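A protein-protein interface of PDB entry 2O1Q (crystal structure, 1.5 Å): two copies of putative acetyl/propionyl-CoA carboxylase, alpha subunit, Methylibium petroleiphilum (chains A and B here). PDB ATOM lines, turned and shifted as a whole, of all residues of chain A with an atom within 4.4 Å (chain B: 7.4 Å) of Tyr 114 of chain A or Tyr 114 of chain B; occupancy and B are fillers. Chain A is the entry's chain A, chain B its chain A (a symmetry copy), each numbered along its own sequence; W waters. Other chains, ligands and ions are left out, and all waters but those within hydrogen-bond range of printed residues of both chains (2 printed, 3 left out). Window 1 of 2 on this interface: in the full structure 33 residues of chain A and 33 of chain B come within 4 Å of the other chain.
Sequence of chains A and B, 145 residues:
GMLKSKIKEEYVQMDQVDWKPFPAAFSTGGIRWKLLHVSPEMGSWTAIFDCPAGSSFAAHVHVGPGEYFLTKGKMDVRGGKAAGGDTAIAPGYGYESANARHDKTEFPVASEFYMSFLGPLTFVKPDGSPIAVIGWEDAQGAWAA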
ATOM      1  N   LEU A  36     -14.937   9.082  24.565  1.00  0.00           N
ATOM      2  CA  LEU A  36     -13.646   8.963  25.222  1.00  0.00           C
ATOM      3  C   LEU A  36     -12.571   9.785  24.522  1.00  0.00           C
ATOM      4  O   LEU A  36     -11.673  10.362  25.175  1.00  0.00           O
ATOM      5  CB  LEU A  36     -13.237   7.516  25.272  1.00  0.00           C
ATOM      6  CG  LEU A  36     -14.143   6.609  26.119  1.00  0.00           C
ATOM      7  CD1 LEU A  36     -13.699   5.138  25.923  1.00  0.00           C
ATOM      8  CD2 LEU A  36     -14.195   7.051  27.594  1.00  0.00           C
ATOM      9  N   THR A  46     -13.630   7.448  19.584  1.00  0.00           N
ATOM     10  CA  THR A  46     -13.682   6.267  20.405  1.00  0.00           C
ATOM     11  C   THR A  46     -14.649   6.557  21.537  1.00  0.00           C
ATOM     12  O   THR A  46     -14.664   7.690  22.102  1.00  0.00           O
ATOM     13  CB  THR A  46     -12.299   6.014  20.988  1.00  0.00           C
ATOM     14  OG1 THR A  46     -11.332   5.877  19.947  1.00  0.00           O
ATOM     15  CG2 THR A  46     -12.285   4.846  21.895  1.00  0.00           C
ATOM     16  N   ALA A  47     -15.487   5.574  21.814  1.00  0.00           N
ATOM     17  CA  ALA A  47     -16.570   5.712  22.762  1.00  0.00           C
ATOM     18  C   ALA A  47     -16.857   4.383  23.376  1.00  0.00           C
ATOM     19  O   ALA A  47     -16.449   3.304  22.817  1.00  0.00           O
ATOM     20  CB  ALA A  47     -17.826   6.304  22.045  1.00  0.00           C
ATOM     21  N   ILE A  48     -17.549   4.412  24.532  1.00  0.00           N
ATOM     22  CA  ILE A  48     -18.071   3.185  25.167  1.00  0.00           C
ATOM     23  C   ILE A  48     -19.566   3.353  25.342  1.00  0.00           C
ATOM     24  O   ILE A  48     -20.066   4.488  25.423  1.00  0.00           O
ATOM     25  CB  ILE A  48     -17.336   2.841  26.492  1.00  0.00           C
ATOM     26  CG1 ILE A  48     -17.731   1.484  27.001  1.00  0.00           C
ATOM     27  CG2 ILE A  48     -17.500   4.008  27.457  1.00  0.00           C
ATOM     28  CD1 ILE A  48     -16.738   0.905  28.066  1.00  0.00           C
ATOM     29  N   GLU A  67     -13.365  -0.967  15.263  1.00  0.00           N
ATOM     30  CA  GLU A  67     -12.992  -2.149  16.053  1.00  0.00           C
ATOM     31  C   GLU A  67     -13.657  -2.059  17.416  1.00  0.00           C
ATOM     32  O   GLU A  67     -13.625  -0.974  18.059  1.00  0.00           O
ATOM     33  CB  GLU A  67     -11.486  -2.171  16.261  1.00  0.00           C
ATOM     34  CG  GLU A  67     -10.733  -2.301  15.022  1.00  0.00           C
ATOM     35  CD  GLU A  67      -9.232  -2.432  15.266  1.00  0.00           C
ATOM     36  OE1 GLU A  67      -8.794  -3.355  15.996  1.00  0.00           O
ATOM     37  OE2 GLU A  67      -8.482  -1.693  14.599  1.00  0.00           O
ATOM     38  N   TYR A  68     -14.258  -3.133  17.884  1.00  0.00           N
ATOM     39  CA  TYR A  68     -14.922  -3.148  19.143  1.00  0.00           C
ATOM     40  C   TYR A  68     -14.441  -4.248  20.065  1.00  0.00           C
ATOM     41  O   TYR A  68     -13.943  -5.270  19.595  1.00  0.00           O
ATOM     42  CB  TYR A  68     -16.441  -3.235  18.996  1.00  0.00           C
ATOM     43  CG  TYR A  68     -16.967  -4.552  18.465  1.00  0.00           C
ATOM     44  CD1 TYR A  68     -17.081  -5.645  19.309  1.00  0.00           C
ATOM     45  CD2 TYR A  68     -17.367  -4.684  17.137  1.00  0.00           C
ATOM     46  CE1 TYR A  68     -17.532  -6.862  18.812  1.00  0.00           C
ATOM     47  CE2 TYR A  68     -17.855  -5.907  16.664  1.00  0.00           C
ATOM     48  CZ  TYR A  68     -17.943  -6.987  17.540  1.00  0.00           C
ATOM     49  OH  TYR A  68     -18.364  -8.213  17.034  1.00  0.00           O
ATOM     50  N   PHE A  69     -14.604  -3.978  21.352  1.00  0.00           N
ATOM     51  CA  PHE A  69     -14.398  -4.885  22.451  1.00  0.00           C
ATOM     52  C   PHE A  69     -15.688  -4.894  23.270  1.00  0.00           C
ATOM     53  O   PHE A  69     -16.033  -3.922  23.965  1.00  0.00           O
ATOM     54  CB  PHE A  69     -13.212  -4.444  23.267  1.00  0.00           C
ATOM     55  CG  PHE A  69     -12.860  -5.315  24.455  1.00  0.00           C
ATOM     56  CD1 PHE A  69     -13.379  -6.585  24.692  1.00  0.00           C
ATOM     57  CD2 PHE A  69     -11.965  -4.807  25.384  1.00  0.00           C
ATOM     58  CE1 PHE A  69     -12.997  -7.299  25.830  1.00  0.00           C
ATOM     59  CE2 PHE A  69     -11.584  -5.512  26.477  1.00  0.00           C
ATOM     60  CZ  PHE A  69     -12.079  -6.759  26.709  1.00  0.00           C
ATOM     61  N   TYR A  93     -14.236  -9.559  20.442  1.00  0.00           N
ATOM     62  CA  TYR A  93     -13.568  -8.532  19.632  1.00  0.00           C
ATOM     63  C   TYR A  93     -14.130  -8.616  18.210  1.00  0.00           C
ATOM     64  O   TYR A  93     -14.333  -9.709  17.697  1.00  0.00           O
ATOM     65  CB  TYR A  93     -12.060  -8.742  19.589  1.00  0.00           C
ATOM     66  CG  TYR A  93     -11.415  -7.937  18.490  1.00  0.00           C
ATOM     67  CD1 TYR A  93     -11.065  -6.620  18.695  1.00  0.00           C
ATOM     68  CD2 TYR A  93     -11.231  -8.463  17.220  1.00  0.00           C
ATOM     69  CE1 TYR A  93     -10.559  -5.859  17.621  1.00  0.00           C
ATOM     70  CE2 TYR A  93     -10.772  -7.712  16.162  1.00  0.00           C
ATOM     71  CZ  TYR A  93     -10.429  -6.405  16.358  1.00  0.00           C
ATOM     72  OH  TYR A  93      -9.958  -5.598  15.340  1.00  0.00           O
ATOM     73  N   PHE A 113     -19.929  -2.177  25.356  1.00  0.00           N
ATOM     74  CA  PHE A 113     -18.869  -2.290  24.343  1.00  0.00           C
ATOM     75  C   PHE A 113     -18.191  -0.985  24.106  1.00  0.00           C
ATOM     76  O   PHE A 113     -18.814   0.103  24.167  1.00  0.00           O
ATOM     77  CB  PHE A 113     -19.319  -2.918  23.011  1.00  0.00           C
ATOM     78  CG  PHE A 113     -20.131  -2.017  22.151  1.00  0.00           C
ATOM     79  CD1 PHE A 113     -21.486  -1.787  22.422  1.00  0.00           C
ATOM     80  CD2 PHE A 113     -19.538  -1.338  21.083  1.00  0.00           C
ATOM     81  CE1 PHE A 113     -22.212  -0.902  21.607  1.00  0.00           C
ATOM     82  CE2 PHE A 113     -20.271  -0.504  20.284  1.00  0.00           C
ATOM     83  CZ  PHE A 113     -21.626  -0.322  20.549  1.00  0.00           C
ATOM     84  N   TYR A 114     -16.896  -1.130  23.881  1.00  0.00           N
ATOM     85  CA  TYR A 114     -15.947  -0.077  23.558  1.00  0.00           C
ATOM     86  C   TYR A 114     -15.679  -0.190  22.073  1.00  0.00           C
ATOM     87  O   TYR A 114     -15.492  -1.302  21.559  1.00  0.00           O
ATOM     88  CB  TYR A 114     -14.672  -0.336  24.403  1.00  0.00           C
ATOM     89  CG  TYR A 114     -13.460   0.505  24.060  1.00  0.00           C
ATOM     90  CD1 TYR A 114     -12.611   0.132  23.068  1.00  0.00           C
ATOM     91  CD2 TYR A 114     -13.117   1.633  24.783  1.00  0.00           C
ATOM     92  CE1 TYR A 114     -11.467   0.823  22.814  1.00  0.00           C
ATOM     93  CE2 TYR A 114     -11.965   2.336  24.527  1.00  0.00           C
ATOM     94  CZ  TYR A 114     -11.157   1.957  23.530  1.00  0.00           C
ATOM     95  OH  TYR A 114      -9.979   2.589  23.244  1.00  0.00           O
ATOM     96  N   MET A 115     -15.724   0.934  21.358  1.00  0.00           N
ATOM     97  CA  MET A 115     -15.469   0.957  19.949  1.00  0.00           C
ATOM     98  C   MET A 115     -14.725   2.167  19.507  1.00  0.00           C
ATOM     99  O   MET A 115     -14.974   3.294  19.962  1.00  0.00           O
ATOM    100  CB  MET A 115     -16.774   0.809  19.159  1.00  0.00           C
ATOM    101  CG  MET A 115     -16.572   0.577  17.715  1.00  0.00           C
ATOM    102  SD  MET A 115     -18.173  -0.261  16.920  1.00  0.00           S
ATOM    103  CE  MET A 115     -17.295  -0.403  15.156  1.00  0.00           C
ATOM    104  N   MET B  14     -12.942 -14.111  22.541  1.00  0.00           N
ATOM    105  CA  MET B  14     -11.672 -13.905  23.218  1.00  0.00           C
ATOM    106  C   MET B  14     -11.406 -14.959  24.290  1.00  0.00           C
ATOM    107  O   MET B  14     -10.255 -15.355  24.444  1.00  0.00           O
ATOM    108  CB  MET B  14     -11.611 -12.484  23.802  1.00  0.00           C
ATOM    109  CG  MET B  14     -11.607 -11.385  22.705  1.00  0.00           C
ATOM    110  SD  MET B  14     -12.063  -9.683  23.356  1.00  0.00           S
ATOM    111  CE  MET B  14     -10.645  -9.733  24.578  1.00  0.00           C
ATOM    112  N   LYS B  34      -3.016 -11.638  23.975  1.00  0.00           N
ATOM    113  CA  LYS B  34      -3.779 -12.239  22.848  1.00  0.00           C
ATOM    114  C   LYS B  34      -3.719 -11.162  21.796  1.00  0.00           C
ATOM    115  O   LYS B  34      -4.168 -10.038  22.034  1.00  0.00           O
ATOM    116  CB  LYS B  34      -5.206 -12.538  23.234  1.00  0.00           C
ATOM    117  CG  LYS B  34      -5.295 -13.501  24.411  1.00  0.00           C
ATOM    118  CD  LYS B  34      -6.744 -13.783  24.787  1.00  0.00           C
ATOM    119  CE  LYS B  34      -6.807 -14.635  26.024  1.00  0.00           C
ATOM    120  NZ  LYS B  34      -8.199 -15.086  26.349  1.00  0.00           N
ATOM    121  N   LEU B  36      -5.411  -9.738  18.657  1.00  0.00           N
ATOM    122  CA  LEU B  36      -6.808  -9.753  18.257  1.00  0.00           C
ATOM    123  C   LEU B  36      -6.983  -9.436  16.778  1.00  0.00           C
ATOM    124  O   LEU B  36      -7.870  -9.998  16.097  1.00  0.00           O
ATOM    125  CB  LEU B  36      -7.582  -8.768  19.091  1.00  0.00           C
ATOM    126  CG  LEU B  36      -7.646  -9.090  20.592  1.00  0.00           C
ATOM    127  CD1 LEU B  36      -8.313  -7.901  21.329  1.00  0.00           C
ATOM    128  CD2 LEU B  36      -8.318 -10.448  20.870  1.00  0.00           C
ATOM    129  N   HIS B  37      -6.110  -8.592  16.246  1.00  0.00           N
ATOM    130  CA  HIS B  37      -6.278  -8.142  14.857  1.00  0.00           C
ATOM    131  C   HIS B  37      -5.002  -7.524  14.332  1.00  0.00           C
ATOM    132  O   HIS B  37      -4.290  -6.802  15.067  1.00  0.00           O
ATOM    133  CB  HIS B  37      -7.439  -7.144  14.732  1.00  0.00           C
ATOM    134  CG  HIS B  37      -7.537  -6.487  13.387  1.00  0.00           C
ATOM    135  ND1 HIS B  37      -8.168  -7.071  12.315  1.00  0.00           N
ATOM    136  CD2 HIS B  37      -7.084  -5.297  12.956  1.00  0.00           C
ATOM    137  CE1 HIS B  37      -8.045  -6.281  11.259  1.00  0.00           C
ATOM    138  NE2 HIS B  37      -7.415  -5.181  11.634  1.00  0.00           N
ATOM    139  N   THR B  46      -4.049  -4.724  17.175  1.00  0.00           N
ATOM    140  CA  THR B  46      -4.832  -4.600  18.377  1.00  0.00           C
ATOM    141  C   THR B  46      -4.654  -5.889  19.155  1.00  0.00           C
ATOM    142  O   THR B  46      -4.626  -7.008  18.561  1.00  0.00           O
ATOM    143  CB  THR B  46      -6.297  -4.451  17.993  1.00  0.00           C
ATOM    144  OG1 THR B  46      -6.481  -3.324  17.138  1.00  0.00           O
ATOM    145  CG2 THR B  46      -7.176  -4.379  19.180  1.00  0.00           C
ATOM    146  N   ALA B  47      -4.466  -5.730  20.453  1.00  0.00           N
ATOM    147  CA  ALA B  47      -4.140  -6.827  21.337  1.00  0.00           C
ATOM    148  C   ALA B  47      -4.670  -6.532  22.701  1.00  0.00           C
ATOM    149  O   ALA B  47      -4.984  -5.335  23.033  1.00  0.00           O
ATOM    150  CB  ALA B  47      -2.594  -7.051  21.352  1.00  0.00           C
ATOM    151  N   ILE B  48      -4.794  -7.594  23.521  1.00  0.00           N
ATOM    152  CA  ILE B  48      -5.125  -7.448  24.953  1.00  0.00           C
ATOM    153  C   ILE B  48      -4.034  -8.126  25.753  1.00  0.00           C
ATOM    154  O   ILE B  48      -3.359  -9.040  25.248  1.00  0.00           O
ATOM    155  CB  ILE B  48      -6.547  -7.974  25.291  1.00  0.00           C
ATOM    156  CG1 ILE B  48      -6.943  -7.618  26.696  1.00  0.00           C
ATOM    157  CG2 ILE B  48      -6.625  -9.447  24.911  1.00  0.00           C
ATOM    158  CD1 ILE B  48      -8.484  -7.733  26.957  1.00  0.00           C
ATOM    159  N   PHE B  49      -3.734  -7.532  26.896  1.00  0.00           N
ATOM    160  CA  PHE B  49      -2.638  -7.927  27.766  1.00  0.00           C
ATOM    161  C   PHE B  49      -3.105  -8.190  29.180  1.00  0.00           C
ATOM    162  O   PHE B  49      -3.951  -7.465  29.706  1.00  0.00           O
ATOM    163  CB  PHE B  49      -1.587  -6.826  27.808  1.00  0.00           C
ATOM    164  CG  PHE B  49      -1.028  -6.456  26.434  1.00  0.00           C
ATOM    165  CD1 PHE B  49      -1.705  -5.590  25.616  1.00  0.00           C
ATOM    166  CD2 PHE B  49       0.145  -7.031  25.953  1.00  0.00           C
ATOM    167  CE1 PHE B  49      -1.216  -5.253  24.391  1.00  0.00           C
ATOM    168  CE2 PHE B  49       0.626  -6.684  24.726  1.00  0.00           C
ATOM    169  CZ  PHE B  49      -0.055  -5.831  23.938  1.00  0.00           C
ATOM    170  N   GLY B  66      -1.763   5.396  19.584  1.00  0.00           N
ATOM    171  CA  GLY B  66      -2.297   4.206  20.209  1.00  0.00           C
ATOM    172  C   GLY B  66      -3.327   4.597  21.222  1.00  0.00           C
ATOM    173  O   GLY B  66      -3.269   5.682  21.775  1.00  0.00           O
ATOM    174  N   GLU B  67      -4.297   3.713  21.455  1.00  0.00           N
ATOM    175  CA  GLU B  67      -5.388   3.986  22.403  1.00  0.00           C
ATOM    176  C   GLU B  67      -5.631   2.744  23.242  1.00  0.00           C
ATOM    177  O   GLU B  67      -5.700   1.614  22.686  1.00  0.00           O
ATOM    178  CB  GLU B  67      -6.663   4.300  21.637  1.00  0.00           C
ATOM    179  CG  GLU B  67      -6.568   5.504  20.823  1.00  0.00           C
ATOM    180  CD  GLU B  67      -7.893   5.856  20.154  1.00  0.00           C
ATOM    181  OE1 GLU B  67      -8.922   6.032  20.853  1.00  0.00           O
ATOM    182  OE2 GLU B  67      -7.864   6.105  18.933  1.00  0.00           O
ATOM    183  N   TYR B  68      -5.762   2.893  24.544  1.00  0.00           N
ATOM    184  CA  TYR B  68      -5.979   1.791  25.420  1.00  0.00           C
ATOM    185  C   TYR B  68      -7.203   1.951  26.295  1.00  0.00           C
ATOM    186  O   TYR B  68      -7.620   3.075  26.570  1.00  0.00           O
ATOM    187  CB  TYR B  68      -4.761   1.498  26.295  1.00  0.00           C
ATOM    188  CG  TYR B  68      -4.449   2.543  27.345  1.00  0.00           C
ATOM    189  CD1 TYR B  68      -5.172   2.576  28.527  1.00  0.00           C
ATOM    190  CD2 TYR B  68      -3.424   3.467  27.158  1.00  0.00           C
ATOM    191  CE1 TYR B  68      -4.907   3.557  29.475  1.00  0.00           C
ATOM    192  CE2 TYR B  68      -3.146   4.424  28.140  1.00  0.00           C
ATOM    193  CZ  TYR B  68      -3.903   4.434  29.311  1.00  0.00           C
ATOM    194  OH  TYR B  68      -3.659   5.435  30.245  1.00  0.00           O
ATOM    195  N   PHE B  69      -7.734   0.802  26.689  1.00  0.00           N
ATOM    196  CA  PHE B  69      -8.791   0.631  27.651  1.00  0.00           C
ATOM    197  C   PHE B  69      -8.277  -0.342  28.711  1.00  0.00           C
ATOM    198  O   PHE B  69      -8.120  -1.554  28.472  1.00  0.00           O
ATOM    199  CB  PHE B  69     -10.032   0.121  26.968  1.00  0.00           C
ATOM    200  CG  PHE B  69     -11.240  -0.093  27.855  1.00  0.00           C
ATOM    201  CD1 PHE B  69     -11.360   0.369  29.162  1.00  0.00           C
ATOM    202  CD2 PHE B  69     -12.304  -0.814  27.332  1.00  0.00           C
ATOM    203  CE1 PHE B  69     -12.516   0.102  29.899  1.00  0.00           C
ATOM    204  CE2 PHE B  69     -13.431  -1.054  28.046  1.00  0.00           C
ATOM    205  CZ  PHE B  69     -13.559  -0.595  29.321  1.00  0.00           C
ATOM    206  N   LEU B  70      -7.883   0.213  29.838  1.00  0.00           N
ATOM    207  CA  LEU B  70      -7.473  -0.559  31.030  1.00  0.00           C
ATOM    208  C   LEU B  70      -8.712  -1.036  31.719  1.00  0.00           C
ATOM    209  O   LEU B  70      -9.469  -0.219  32.284  1.00  0.00           O
ATOM    210  CB  LEU B  70      -6.649   0.266  31.963  1.00  0.00           C
ATOM    211  CG  LEU B  70      -6.069  -0.274  33.266  1.00  0.00           C
ATOM    212  CD1 LEU B  70      -4.949  -1.226  32.841  1.00  0.00           C
ATOM    213  CD2 LEU B  70      -5.620   0.862  34.197  1.00  0.00           C
ATOM    214  N   THR B  71      -8.987  -2.347  31.638  1.00  0.00           N
ATOM    215  CA  THR B  71     -10.234  -2.884  32.163  1.00  0.00           C
ATOM    216  C   THR B  71     -10.075  -3.339  33.591  1.00  0.00           C
ATOM    217  O   THR B  71     -11.075  -3.490  34.310  1.00  0.00           O
ATOM    218  CB  THR B  71     -10.708  -4.040  31.328  1.00  0.00           C
ATOM    219  OG1 THR B  71      -9.656  -4.986  31.278  1.00  0.00           O
ATOM    220  CG2 THR B  71     -11.027  -3.618  29.896  1.00  0.00           C
ATOM    221  N   GLY B  92     -10.055   2.789  32.836  1.00  0.00           N
ATOM    222  CA  GLY B  92      -9.311   3.950  32.321  1.00  0.00           C
ATOM    223  C   GLY B  92      -9.097   3.877  30.830  1.00  0.00           C
ATOM    224  O   GLY B  92      -8.838   2.783  30.294  1.00  0.00           O
ATOM    225  N   TYR B  93      -9.164   5.038  30.171  1.00  0.00           N
ATOM    226  CA  TYR B  93      -8.904   5.186  28.733  1.00  0.00           C
ATOM    227  C   TYR B  93      -7.686   6.101  28.568  1.00  0.00           C
ATOM    228  O   TYR B  93      -7.565   7.090  29.278  1.00  0.00           O
ATOM    229  CB  TYR B  93     -10.094   5.799  28.006  1.00  0.00           C
ATOM    230  CG  TYR B  93      -9.717   6.288  26.631  1.00  0.00           C
ATOM    231  CD1 TYR B  93      -9.708   5.427  25.556  1.00  0.00           C
ATOM    232  CD2 TYR B  93      -9.288   7.590  26.418  1.00  0.00           C
ATOM    233  CE1 TYR B  93      -9.252   5.883  24.302  1.00  0.00           C
ATOM    234  CE2 TYR B  93      -8.809   8.027  25.204  1.00  0.00           C
ATOM    235  CZ  TYR B  93      -8.792   7.176  24.136  1.00  0.00           C
ATOM    236  OH  TYR B  93      -8.328   7.553  22.891  1.00  0.00           O
ATOM    237  N   GLY B  94      -6.796   5.794  27.631  1.00  0.00           N
ATOM    238  CA  GLY B  94      -5.688   6.652  27.305  1.00  0.00           C
ATOM    239  C   GLY B  94      -5.466   6.789  25.825  1.00  0.00           C
ATOM    240  O   GLY B  94      -5.644   5.805  25.091  1.00  0.00           O
ATOM    241  N   GLU B 112      -5.311  -5.699  33.261  1.00  0.00           N
ATOM    242  CA  GLU B 112      -5.681  -6.155  31.941  1.00  0.00           C
ATOM    243  C   GLU B 112      -5.971  -4.914  31.169  1.00  0.00           C
ATOM    244  O   GLU B 112      -6.661  -4.015  31.680  1.00  0.00           O
ATOM    245  CB  GLU B 112      -6.955  -6.972  31.962  1.00  0.00           C
ATOM    246  CG  GLU B 112      -7.356  -7.529  30.594  1.00  0.00           C
ATOM    247  CD  GLU B 112      -8.667  -8.273  30.649  1.00  0.00           C
ATOM    248  OE1 GLU B 112      -9.744  -7.612  30.718  1.00  0.00           O
ATOM    249  OE2 GLU B 112      -8.598  -9.514  30.601  1.00  0.00           O
ATOM    250  N   PHE B 113      -5.419  -4.810  29.972  1.00  0.00           N
ATOM    251  CA  PHE B 113      -5.682  -3.689  29.057  1.00  0.00           C
ATOM    252  C   PHE B 113      -5.674  -4.125  27.633  1.00  0.00           C
ATOM    253  O   PHE B 113      -4.908  -5.031  27.225  1.00  0.00           O
ATOM    254  CB  PHE B 113      -4.764  -2.469  29.257  1.00  0.00           C
ATOM    255  CG  PHE B 113      -3.382  -2.649  28.737  1.00  0.00           C
ATOM    256  CD1 PHE B 113      -2.434  -3.393  29.450  1.00  0.00           C
ATOM    257  CD2 PHE B 113      -3.022  -2.119  27.495  1.00  0.00           C
ATOM    258  CE1 PHE B 113      -1.148  -3.569  28.911  1.00  0.00           C
ATOM    259  CE2 PHE B 113      -1.755  -2.278  27.003  1.00  0.00           C
ATOM    260  CZ  PHE B 113      -0.818  -2.988  27.749  1.00  0.00           C
ATOM    261  N   TYR B 114      -6.578  -3.485  26.910  1.00  0.00           N
ATOM    262  CA  TYR B 114      -6.803  -3.621  25.481  1.00  0.00           C
ATOM    263  C   TYR B 114      -6.192  -2.395  24.838  1.00  0.00           C
ATOM    264  O   TYR B 114      -6.373  -1.276  25.338  1.00  0.00           O
ATOM    265  CB  TYR B 114      -8.338  -3.691  25.265  1.00  0.00           C
ATOM    266  CG  TYR B 114      -8.815  -3.602  23.830  1.00  0.00           C
ATOM    267  CD1 TYR B 114      -9.009  -2.398  23.233  1.00  0.00           C
ATOM    268  CD2 TYR B 114      -9.154  -4.724  23.096  1.00  0.00           C
ATOM    269  CE1 TYR B 114      -9.530  -2.301  21.980  1.00  0.00           C
ATOM    270  CE2 TYR B 114      -9.677  -4.630  21.829  1.00  0.00           C
ATOM    271  CZ  TYR B 114      -9.837  -3.431  21.257  1.00  0.00           C
ATOM    272  OH  TYR B 114     -10.384  -3.264  20.015  1.00  0.00           O
ATOM    273  N   MET B 115      -5.413  -2.588  23.774  1.00  0.00           N
ATOM    274  CA  MET B 115      -4.795  -1.506  23.069  1.00  0.00           C
ATOM    275  C   MET B 115      -4.748  -1.715  21.597  1.00  0.00           C
ATOM    276  O   MET B 115      -4.481  -2.820  21.098  1.00  0.00           O
ATOM    277  CB  MET B 115      -3.390  -1.233  23.619  1.00  0.00           C
ATOM    278  CG  MET B 115      -2.788   0.019  23.115  1.00  0.00           C
ATOM    279  SD  MET B 115      -1.361   0.635  24.332  1.00  0.00           S
ATOM    280  CE  MET B 115      -1.065   2.265  23.254  1.00  0.00           C
ATOM    281  N   SER B 116      -4.972  -0.617  20.893  1.00  0.00           N
ATOM    282  CA  SER B 116      -4.842  -0.556  19.470  1.00  0.00           C
ATOM    283  C   SER B 116      -3.652   0.365  19.197  1.00  0.00           C
ATOM    284  O   SER B 116      -3.389   1.317  19.935  1.00  0.00           O
ATOM    285  CB  SER B 116      -6.138  -0.059  18.851  1.00  0.00           C
ATOM    286  OG  SER B 116      -6.246  -0.470  17.501  1.00  0.00           O
ATOM    287  N   PHE B 117      -2.917   0.007  18.155  1.00  0.00           N
ATOM    288  CA  PHE B 117      -1.695   0.686  17.720  1.00  0.00           C
ATOM    289  C   PHE B 117      -1.734   0.988  16.251  1.00  0.00           C
ATOM    290  O   PHE B 117      -2.001   0.099  15.452  1.00  0.00           O
ATOM    291  CB  PHE B 117      -0.483  -0.205  17.938  1.00  0.00           C
ATOM    292  CG  PHE B 117      -0.360  -0.786  19.345  1.00  0.00           C
ATOM    293  CD1 PHE B 117      -0.945  -2.013  19.647  1.00  0.00           C
ATOM    294  CD2 PHE B 117       0.404  -0.152  20.308  1.00  0.00           C
ATOM    295  CE1 PHE B 117      -0.847  -2.553  20.920  1.00  0.00           C
ATOM    296  CE2 PHE B 117       0.503  -0.678  21.638  1.00  0.00           C
ATOM    297  CZ  PHE B 117      -0.058  -1.905  21.910  1.00  0.00           C
HETATM  298  O   HOH W   1      -9.928   7.617  17.921  1.00  0.00           O
HETATM  299  O   HOH W   2      -5.875  -2.517  14.295  1.00  0.00           O
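The side-chain hydroxyl (OG1) of Thr 46 of chain A lies within hydrogen-bond range of the side-chain carboxylate (OE1) of Glu 67 of chain B, 2.6 Å away. OE1 of Glu 67 of chain A sits at hydrogen-bond distance from OG1 of Thr 46 of chain B (2.6 Å). The side-chain sulfur (SD) of Met 14 of chain B sits at hydrogen-bond distance from the backbone NH (N) of Tyr 93 of chain A, at 3.6 Å.
Hydrophobic or aromatic side chains of chain B that line the printed part of chain A: Met 14, Leu 36, His 37, Ile 48, Phe 69, Tyr 93 and Tyr 114.
Of the printed residues of chain A, Phe 69 of chain B touches Ile 48 and Tyr 114. Of the printed residues of chain A, Tyr 93 of chain B touches Leu 36 (3.7 Å) and Tyr 114 (3.5 Å). Tyr 114 of chain B touches three residues of chain A. Phe 117 of chain B touches none of the printed residues of chain A. The nearest residue of chain B that does not touch Tyr 114 of chain A is Glu 67 of chain B (4.1 Å). The nearest residue of chain A that does not touch Tyr 114 of chain B is Glu 67 of chain A (4.1 Å). The nearest printed residue of chain A that does not touch Thr 71 of chain B is Tyr 114 of chain A (7.4 Å).
The backbone NH (N) of Lys 34 of chain B lies within hydrogen-bond range of the backbone carbonyl oxygen (O) of Ile 48 of chain B (2.9 Å). O of His 37 of chain B is in hydrogen-bond range of N of Thr 46 of chain B, 3.0 Å away. OG of Ser 116 of chain B sits at hydrogen-bond distance from OG1 of Thr 46 of chain B, at 2.9 Å. The side-chain carboxylate of Glu 67 of chain B lies within hydrogen-bond range of the side-chain hydroxyl of Tyr 93 of chain B (2.6 Å). The side-chain hydroxyl (OG1) of Thr 71 of chain B lies within hydrogen-bond range of the side-chain carboxylate (OE1) of Glu 112 of chain B, 2.7 Å away.
Leu 36 of chain A touches Tyr 93 of chain B, and with the chains exchanged Tyr 93 of chain A touches Leu 36 of chain B. Thr 46 of chain A touches Glu 67 of chain B, and with the chains exchanged Glu 67 of chain A touches Thr 46 of chain B. Ile 48 of chain A touches Phe 69 of chain B, and with the chains exchanged Phe 69 of chain A touches Ile 48 of chain B. Tyr 93 of chain A touches Tyr 114 of chain B, and with the chains exchanged Tyr 114 of chain A touches Tyr 93 of chain B. Of the 17 pairs that touch across the chains among the printed residues, 11 have their exchanged pair printed and touching as well.
Water W1 lies within hydrogen-bond range of OE2 of Glu 67 of chain B (2.8 Å) and OG1 of Thr 46 of chain A (3.0 Å). Water W2 lies within hydrogen-bond range of OE2 of Glu 67 of chain A (2.8 Å) and OG1 of Thr 46 of chain B (3.0 Å).
Among the printed residues, pairs that only touch across the chains: Tyr 93 of chain A with His 37 of chain B (3.0 Å), Tyr 93 of chain A with Tyr 114 of chain B (3.5 Å), Tyr 114 of chain A with Tyr 93 of chain B (3.5 Å), Phe 69 of chain A with Met 14 of chain B (3.6 Å), Phe 69 of chain A with Tyr 114 of chain B (3.6 Å), Tyr 114 of chain A with Phe 69 of chain B (3.6 Å), Tyr 93 of chain A with Leu 36 of chain B (3.7 Å), Leu 36 of chain A with Tyr 93 of chain B (3.7 Å), Ile 48 of chain A with Phe 69 of chain B (3.7 Å), Phe 69 of chain A with Ile 48 of chain B (3.7 Å), Tyr 114 of chain A with Tyr 114 of chain B (3.8 Å), Glu 67 of chain A with Ser 116 of chain B (3.9 Å), Phe 69 of chain A with Thr 71 of chain B (3.9 Å) and Glu 67 of chain A with His 37 of chain B (3.99 Å).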
